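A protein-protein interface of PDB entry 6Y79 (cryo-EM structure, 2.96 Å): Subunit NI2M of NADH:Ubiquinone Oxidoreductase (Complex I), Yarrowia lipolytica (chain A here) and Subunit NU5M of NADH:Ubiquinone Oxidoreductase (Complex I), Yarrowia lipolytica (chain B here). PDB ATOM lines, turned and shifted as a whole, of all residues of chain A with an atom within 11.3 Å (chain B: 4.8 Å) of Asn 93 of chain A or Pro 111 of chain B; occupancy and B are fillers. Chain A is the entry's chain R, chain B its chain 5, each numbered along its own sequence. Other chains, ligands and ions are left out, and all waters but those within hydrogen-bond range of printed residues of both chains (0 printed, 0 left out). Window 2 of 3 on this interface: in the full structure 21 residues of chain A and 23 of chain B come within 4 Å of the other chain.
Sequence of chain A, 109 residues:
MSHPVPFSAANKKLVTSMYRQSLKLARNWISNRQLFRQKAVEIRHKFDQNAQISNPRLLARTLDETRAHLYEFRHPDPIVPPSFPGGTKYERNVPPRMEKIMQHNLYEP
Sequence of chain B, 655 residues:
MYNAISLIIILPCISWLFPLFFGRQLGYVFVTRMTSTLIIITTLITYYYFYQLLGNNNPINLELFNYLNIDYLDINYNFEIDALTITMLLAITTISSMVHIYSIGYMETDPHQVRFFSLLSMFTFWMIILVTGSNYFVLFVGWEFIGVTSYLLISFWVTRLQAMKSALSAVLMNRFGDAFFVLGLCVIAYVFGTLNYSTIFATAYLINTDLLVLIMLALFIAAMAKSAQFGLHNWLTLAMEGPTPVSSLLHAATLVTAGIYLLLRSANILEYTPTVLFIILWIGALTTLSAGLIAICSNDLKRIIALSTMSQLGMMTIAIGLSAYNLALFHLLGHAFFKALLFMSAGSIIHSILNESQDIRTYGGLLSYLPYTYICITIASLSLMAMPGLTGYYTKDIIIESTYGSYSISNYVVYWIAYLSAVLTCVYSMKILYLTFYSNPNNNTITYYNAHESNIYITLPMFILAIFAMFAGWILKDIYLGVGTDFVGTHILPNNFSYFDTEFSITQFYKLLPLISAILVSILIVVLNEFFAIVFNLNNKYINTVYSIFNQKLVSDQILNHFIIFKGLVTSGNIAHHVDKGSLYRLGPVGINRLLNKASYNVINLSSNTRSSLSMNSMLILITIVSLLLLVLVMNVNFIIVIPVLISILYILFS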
ATOM      1  N   PRO A  82      27.764  13.528  -4.044  1.00  0.00           N
ATOM      2  CA  PRO A  82      27.359  12.536  -5.048  1.00  0.00           C
ATOM      3  C   PRO A  82      27.446  13.009  -6.485  1.00  0.00           C
ATOM      4  O   PRO A  82      27.728  12.193  -7.368  1.00  0.00           O
ATOM      5  CB  PRO A  82      25.914  12.225  -4.647  1.00  0.00           C
ATOM      6  CG  PRO A  82      25.504  13.410  -3.908  1.00  0.00           C
ATOM      7  CD  PRO A  82      26.663  13.851  -3.136  1.00  0.00           C
ATOM      8  N   SER A  83      27.270  14.296  -6.752  1.00  0.00           N
ATOM      9  CA  SER A  83      27.292  14.796  -8.121  1.00  0.00           C
ATOM     10  C   SER A  83      28.700  15.021  -8.656  1.00  0.00           C
ATOM     11  O   SER A  83      28.851  15.621  -9.722  1.00  0.00           O
ATOM     12  CB  SER A  83      26.490  16.092  -8.216  1.00  0.00           C
ATOM     13  OG  SER A  83      27.124  17.128  -7.494  1.00  0.00           O
ATOM     14  N   PHE A  84      29.717  14.548  -7.952  1.00  0.00           N
ATOM     15  CA  PHE A  84      31.128  14.741  -8.234  1.00  0.00           C
ATOM     16  C   PHE A  84      31.774  13.384  -8.500  1.00  0.00           C
ATOM     17  O   PHE A  84      31.233  12.359  -8.072  1.00  0.00           O
ATOM     18  CB  PHE A  84      31.763  15.467  -7.039  1.00  0.00           C
ATOM     19  CG  PHE A  84      31.386  16.908  -6.963  1.00  0.00           C
ATOM     20  CD1 PHE A  84      30.927  17.585  -8.087  1.00  0.00           C
ATOM     21  CD2 PHE A  84      31.469  17.586  -5.779  1.00  0.00           C
ATOM     22  CE1 PHE A  84      30.565  18.909  -8.014  1.00  0.00           C
ATOM     23  CE2 PHE A  84      31.110  18.892  -5.715  1.00  0.00           C
ATOM     24  CZ  PHE A  84      30.661  19.561  -6.824  1.00  0.00           C
ATOM     25  N   GLY A  87      31.192  10.155  -6.722  1.00  0.00           N
ATOM     26  CA  GLY A  87      29.917   9.987  -6.061  1.00  0.00           C
ATOM     27  C   GLY A  87      28.880   9.243  -6.876  1.00  0.00           C
ATOM     28  O   GLY A  87      29.129   8.745  -7.970  1.00  0.00           O
ATOM     29  N   THR A  88      27.675   9.201  -6.313  1.00  0.00           N
ATOM     30  CA  THR A  88      26.583   8.375  -6.798  1.00  0.00           C
ATOM     31  C   THR A  88      25.658   9.093  -7.768  1.00  0.00           C
ATOM     32  O   THR A  88      24.976   8.427  -8.548  1.00  0.00           O
ATOM     33  CB  THR A  88      25.760   7.871  -5.613  1.00  0.00           C
ATOM     34  OG1 THR A  88      24.994   8.957  -5.078  1.00  0.00           O
ATOM     35  CG2 THR A  88      26.675   7.353  -4.535  1.00  0.00           C
ATOM     36  N   LYS A  89      25.594  10.420  -7.722  1.00  0.00           N
ATOM     37  CA  LYS A  89      24.798  11.211  -8.646  1.00  0.00           C
ATOM     38  C   LYS A  89      25.607  11.650  -9.852  1.00  0.00           C
ATOM     39  O   LYS A  89      25.124  12.447 -10.657  1.00  0.00           O
ATOM     40  CB  LYS A  89      24.232  12.439  -7.926  1.00  0.00           C
ATOM     41  CG  LYS A  89      22.862  12.917  -8.370  1.00  0.00           C
ATOM     42  CD  LYS A  89      22.717  14.404  -8.079  1.00  0.00           C
ATOM     43  CE  LYS A  89      21.563  15.007  -8.836  1.00  0.00           C
ATOM     44  NZ  LYS A  89      20.293  14.427  -8.342  1.00  0.00           N
ATOM     45  N   TYR A  90      26.830  11.155  -9.987  1.00  0.00           N
ATOM     46  CA  TYR A  90      27.724  11.615 -11.037  1.00  0.00           C
ATOM     47  C   TYR A  90      27.308  11.010 -12.365  1.00  0.00           C
ATOM     48  O   TYR A  90      27.225   9.785 -12.487  1.00  0.00           O
ATOM     49  CB  TYR A  90      29.159  11.237 -10.697  1.00  0.00           C
ATOM     50  CG  TYR A  90      30.189  11.702 -11.694  1.00  0.00           C
ATOM     51  CD1 TYR A  90      30.412  13.053 -11.914  1.00  0.00           C
ATOM     52  CD2 TYR A  90      30.960  10.792 -12.394  1.00  0.00           C
ATOM     53  CE1 TYR A  90      31.359  13.480 -12.816  1.00  0.00           C
ATOM     54  CE2 TYR A  90      31.908  11.211 -13.298  1.00  0.00           C
ATOM     55  CZ  TYR A  90      32.103  12.555 -13.503  1.00  0.00           C
ATOM     56  OH  TYR A  90      33.049  12.973 -14.406  1.00  0.00           O
ATOM     57  N   GLU A  91      27.026  11.881 -13.341  1.00  0.00           N
ATOM     58  CA  GLU A  91      26.616  11.521 -14.704  1.00  0.00           C
ATOM     59  C   GLU A  91      25.336  10.693 -14.721  1.00  0.00           C
ATOM     60  O   GLU A  91      25.266   9.639 -15.349  1.00  0.00           O
ATOM     61  CB  GLU A  91      27.730  10.796 -15.456  1.00  0.00           C
ATOM     62  CG  GLU A  91      28.974  11.602 -15.648  1.00  0.00           C
ATOM     63  CD  GLU A  91      30.077  10.799 -16.292  1.00  0.00           C
ATOM     64  OE1 GLU A  91      29.923   9.565 -16.413  1.00  0.00           O
ATOM     65  OE2 GLU A  91      31.100  11.400 -16.682  1.00  0.00           O
ATOM     66  N   ARG A  92      24.305  11.178 -14.037  1.00  0.00           N
ATOM     67  CA  ARG A  92      23.022  10.499 -14.145  1.00  0.00           C
ATOM     68  C   ARG A  92      22.299  10.903 -15.423  1.00  0.00           C
ATOM     69  O   ARG A  92      22.046  10.066 -16.295  1.00  0.00           O
ATOM     70  CB  ARG A  92      22.168  10.772 -12.914  1.00  0.00           C
ATOM     71  CG  ARG A  92      22.444   9.791 -11.813  1.00  0.00           C
ATOM     72  CD  ARG A  92      21.697  10.141 -10.562  1.00  0.00           C
ATOM     73  NE  ARG A  92      20.299   9.751 -10.629  1.00  0.00           N
ATOM     74  CZ  ARG A  92      19.398  10.093  -9.721  1.00  0.00           C
ATOM     75  NH1 ARG A  92      19.755  10.837  -8.694  1.00  0.00           N
ATOM     76  NH2 ARG A  92      18.139   9.704  -9.835  1.00  0.00           N
ATOM     77  N   ASN A  93      21.983  12.183 -15.570  1.00  0.00           N
ATOM     78  CA  ASN A  93      21.370  12.680 -16.795  1.00  0.00           C
ATOM     79  C   ASN A  93      22.260  13.777 -17.352  1.00  0.00           C
ATOM     80  O   ASN A  93      22.034  14.966 -17.122  1.00  0.00           O
ATOM     81  CB  ASN A  93      19.990  13.147 -16.534  1.00  0.00           C
ATOM     82  CG  ASN A  93      19.031  12.000 -16.323  1.00  0.00           C
ATOM     83  OD1 ASN A  93      18.292  11.965 -15.345  1.00  0.00           O
ATOM     84  ND2 ASN A  93      19.043  11.046 -17.245  1.00  0.00           N
ATOM     85  N   VAL A  94      23.285  13.361 -18.084  1.00  0.00           N
ATOM     86  CA  VAL A  94      24.136  14.267 -18.838  1.00  0.00           C
ATOM     87  C   VAL A  94      23.272  14.847 -19.946  1.00  0.00           C
ATOM     88  O   VAL A  94      22.692  14.078 -20.725  1.00  0.00           O
ATOM     89  CB  VAL A  94      25.363  13.537 -19.399  1.00  0.00           C
ATOM     90  CG1 VAL A  94      26.105  14.418 -20.386  1.00  0.00           C
ATOM     91  CG2 VAL A  94      26.266  13.094 -18.269  1.00  0.00           C
ATOM     92  N   PRO A  95      23.108  16.164 -20.027  1.00  0.00           N
ATOM     93  CA  PRO A  95      22.320  16.741 -21.106  1.00  0.00           C
ATOM     94  C   PRO A  95      23.031  16.568 -22.432  1.00  0.00           C
ATOM     95  O   PRO A  95      24.237  16.831 -22.534  1.00  0.00           O
ATOM     96  CB  PRO A  95      22.217  18.222 -20.713  1.00  0.00           C
ATOM     97  CG  PRO A  95      22.520  18.258 -19.266  1.00  0.00           C
ATOM     98  CD  PRO A  95      23.532  17.187 -19.061  1.00  0.00           C
ATOM     99  N   PRO A  96      22.331  16.081 -23.454  1.00  0.00           N
ATOM    100  CA  PRO A  96      22.968  15.913 -24.761  1.00  0.00           C
ATOM    101  C   PRO A  96      23.267  17.261 -25.390  1.00  0.00           C
ATOM    102  O   PRO A  96      22.515  18.223 -25.219  1.00  0.00           O
ATOM    103  CB  PRO A  96      21.922  15.139 -25.565  1.00  0.00           C
ATOM    104  CG  PRO A  96      20.637  15.462 -24.908  1.00  0.00           C
ATOM    105  CD  PRO A  96      20.929  15.637 -23.460  1.00  0.00           C
ATOM    106  N   ARG A  97      24.390  17.338 -26.093  1.00  0.00           N
ATOM    107  CA  ARG A  97      24.750  18.588 -26.736  1.00  0.00           C
ATOM    108  C   ARG A  97      23.844  18.828 -27.938  1.00  0.00           C
ATOM    109  O   ARG A  97      23.355  17.886 -28.567  1.00  0.00           O
ATOM    110  CB  ARG A  97      26.224  18.577 -27.139  1.00  0.00           C
ATOM    111  CG  ARG A  97      26.576  17.649 -28.269  1.00  0.00           C
ATOM    112  CD  ARG A  97      28.074  17.548 -28.441  1.00  0.00           C
ATOM    113  NE  ARG A  97      28.710  16.928 -27.285  1.00  0.00           N
ATOM    114  CZ  ARG A  97      28.836  15.616 -27.114  1.00  0.00           C
ATOM    115  NH1 ARG A  97      28.365  14.772 -28.019  1.00  0.00           N
ATOM    116  NH2 ARG A  97      29.436  15.146 -26.032  1.00  0.00           N
ATOM    117  N   THR B 109      10.842  13.660 -11.122  1.00  0.00           N
ATOM    118  CA  THR B 109      11.596  14.608 -11.916  1.00  0.00           C
ATOM    119  C   THR B 109      12.554  13.933 -12.877  1.00  0.00           C
ATOM    120  O   THR B 109      13.212  14.624 -13.658  1.00  0.00           O
ATOM    121  CB  THR B 109      12.359  15.559 -10.996  1.00  0.00           C
ATOM    122  OG1 THR B 109      12.982  16.584 -11.778  1.00  0.00           O
ATOM    123  CG2 THR B 109      13.410  14.799 -10.208  1.00  0.00           C
ATOM    124  N   ASP B 110      12.657  12.610 -12.823  1.00  0.00           N
ATOM    125  CA  ASP B 110      13.459  11.886 -13.785  1.00  0.00           C
ATOM    126  C   ASP B 110      12.772  11.929 -15.145  1.00  0.00           C
ATOM    127  O   ASP B 110      11.542  11.893 -15.220  1.00  0.00           O
ATOM    128  CB  ASP B 110      13.649  10.441 -13.336  1.00  0.00           C
ATOM    129  CG  ASP B 110      14.642   9.690 -14.194  1.00  0.00           C
ATOM    130  OD1 ASP B 110      15.859   9.897 -14.012  1.00  0.00           O
ATOM    131  OD2 ASP B 110      14.210   8.902 -15.055  1.00  0.00           O
ATOM    132  N   PRO B 111      13.545  12.060 -16.237  1.00  0.00           N
ATOM    133  CA  PRO B 111      12.936  12.086 -17.572  1.00  0.00           C
ATOM    134  C   PRO B 111      12.219  10.804 -17.948  1.00  0.00           C
ATOM    135  O   PRO B 111      11.002  10.806 -18.151  1.00  0.00           O
ATOM    136  CB  PRO B 111      14.133  12.321 -18.498  1.00  0.00           C
ATOM    137  CG  PRO B 111      15.147  12.927 -17.675  1.00  0.00           C
ATOM    138  CD  PRO B 111      14.960  12.457 -16.278  1.00  0.00           C
ATOM    139  N   HIS B 112      12.936   9.688 -17.929  1.00  0.00           N
ATOM    140  CA  HIS B 112      12.603   8.524 -18.740  1.00  0.00           C
ATOM    141  C   HIS B 112      11.752   7.522 -18.005  1.00  0.00           C
ATOM    142  O   HIS B 112      11.992   6.323 -18.118  1.00  0.00           O
ATOM    143  CB  HIS B 112      13.883   7.867 -19.234  1.00  0.00           C
ATOM    144  CG  HIS B 112      14.779   8.784 -20.001  1.00  0.00           C
ATOM    145  ND1 HIS B 112      14.406   9.365 -21.189  1.00  0.00           N
ATOM    146  CD2 HIS B 112      16.043   9.197 -19.761  1.00  0.00           C
ATOM    147  CE1 HIS B 112      15.397  10.106 -21.644  1.00  0.00           C
ATOM    148  NE2 HIS B 112      16.403  10.021 -20.797  1.00  0.00           N
ATOM    149  N   GLN B 113      10.774   7.963 -17.223  1.00  0.00           N
ATOM    150  CA  GLN B 113      10.051   7.011 -16.401  1.00  0.00           C
ATOM    151  C   GLN B 113       9.032   6.170 -17.161  1.00  0.00           C
ATOM    152  O   GLN B 113       8.540   5.199 -16.584  1.00  0.00           O
ATOM    153  CB  GLN B 113       9.386   7.710 -15.214  1.00  0.00           C
ATOM    154  CG  GLN B 113       8.681   9.004 -15.479  1.00  0.00           C
ATOM    155  CD  GLN B 113       8.075   9.542 -14.207  1.00  0.00           C
ATOM    156  OE1 GLN B 113       8.247   8.960 -13.145  1.00  0.00           O
ATOM    157  NE2 GLN B 113       7.352  10.643 -14.305  1.00  0.00           N
ATOM    158  N   TRP B 157      20.509   4.420 -16.068  1.00  0.00           N
ATOM    159  CA  TRP B 157      21.253   5.595 -16.501  1.00  0.00           C
ATOM    160  C   TRP B 157      22.406   5.107 -17.351  1.00  0.00           C
ATOM    161  O   TRP B 157      23.465   4.741 -16.842  1.00  0.00           O
ATOM    162  CB  TRP B 157      21.705   6.432 -15.318  1.00  0.00           C
ATOM    163  CG  TRP B 157      20.537   7.060 -14.719  1.00  0.00           C
ATOM    164  CD1 TRP B 157      19.775   8.042 -15.264  1.00  0.00           C
ATOM    165  CD2 TRP B 157      19.944   6.735 -13.471  1.00  0.00           C
ATOM    166  NE1 TRP B 157      18.742   8.356 -14.427  1.00  0.00           N
ATOM    167  CE2 TRP B 157      18.825   7.563 -13.316  1.00  0.00           C
ATOM    168  CE3 TRP B 157      20.256   5.827 -12.465  1.00  0.00           C
ATOM    169  CZ2 TRP B 157      18.019   7.513 -12.197  1.00  0.00           C
ATOM    170  CZ3 TRP B 157      19.456   5.780 -11.354  1.00  0.00           C
ATOM    171  CH2 TRP B 157      18.353   6.619 -11.225  1.00  0.00           C
ATOM    172  N   THR B 159      24.111   6.898 -19.272  1.00  0.00           N
ATOM    173  CA  THR B 159      25.171   7.898 -19.254  1.00  0.00           C
ATOM    174  C   THR B 159      26.206   7.590 -18.187  1.00  0.00           C
ATOM    175  O   THR B 159      27.385   7.918 -18.346  1.00  0.00           O
ATOM    176  CB  THR B 159      24.565   9.275 -19.017  1.00  0.00           C
ATOM    177  OG1 THR B 159      23.901   9.284 -17.749  1.00  0.00           O
ATOM    178  CG2 THR B 159      23.553   9.585 -20.093  1.00  0.00           C
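OG1 of Thr 159 of chain B is in hydrogen-bond range of O of Glu 91 of chain A (2.8 Å). The backbone carbonyl oxygen (O) of Arg 92 of chain A sits at hydrogen-bond distance from the side-chain hydroxyl (OG1) of Thr 159 of chain B (2.5 Å). OD1 of Asn 93 of chain A sits close to OD1 of Asp 110 of chain B (3.5 Å).
The side-chain hydroxyl of Tyr 90 of chain A lies within hydrogen-bond range of the side-chain carboxylate of Glu 91 of chain A. The side-chain carboxylate (OD2) of Asp 110 of chain B is in hydrogen-bond range of the backbone NH (N) of His 112 of chain B, at 3.2 Å. The indole nitrogen (NE1) of Trp 157 of chain B is in hydrogen-bond range of the side-chain carboxylate (OD1) of Asp 110 of chain B (3.3 Å).
Among the printed residues, merely in contact across the chains: Arg 92 of chain A with Trp 157 of chain B (3.2 Å), Asn 93 of chain A with Pro 111 of chain B (3.5 Å) and Asn 93 of chain A with Trp 157 of chain B (3.7 Å).
Of chain B, only Asp 110 (3.5 Å), Pro 111 (3.5 Å) and Trp 157 (3.7 Å) come within 4 Å of Asn 93 of chain A. Pro 111 of chain B touches just one residue of chain A: Asn 93 (3.5 Å). No residue of chain A comes within 4 Å of Thr 109 of chain B. Of chain A, only Asn 93 (3.5 Å) comes within 4 Å of Asp 110 of chain B. No residue of chain A comes within 4 Å of His 112 of chain B. Of the printed residues of chain A, Thr 159 of chain B touches Glu 91 and Arg 92. Of the printed residues of chain A, Trp 157 of chain B touches Arg 92 and Asn 93. Tyr 90 of chain A touches none of the printed residues of chain B. Ser 83 of chain A touches none of the printed residues of chain B. The nearest residue of chain B that does not touch Asn 93 of chain A is Thr 159 of chain B (4.1 Å).
Of the 14 printed residues of chain A, 3 touch a printed residue of chain B. Among the printed residues, no Asp or Glu carboxylate lies within 4 Å of a Lys or Arg side-chain nitrogen of the other chain.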
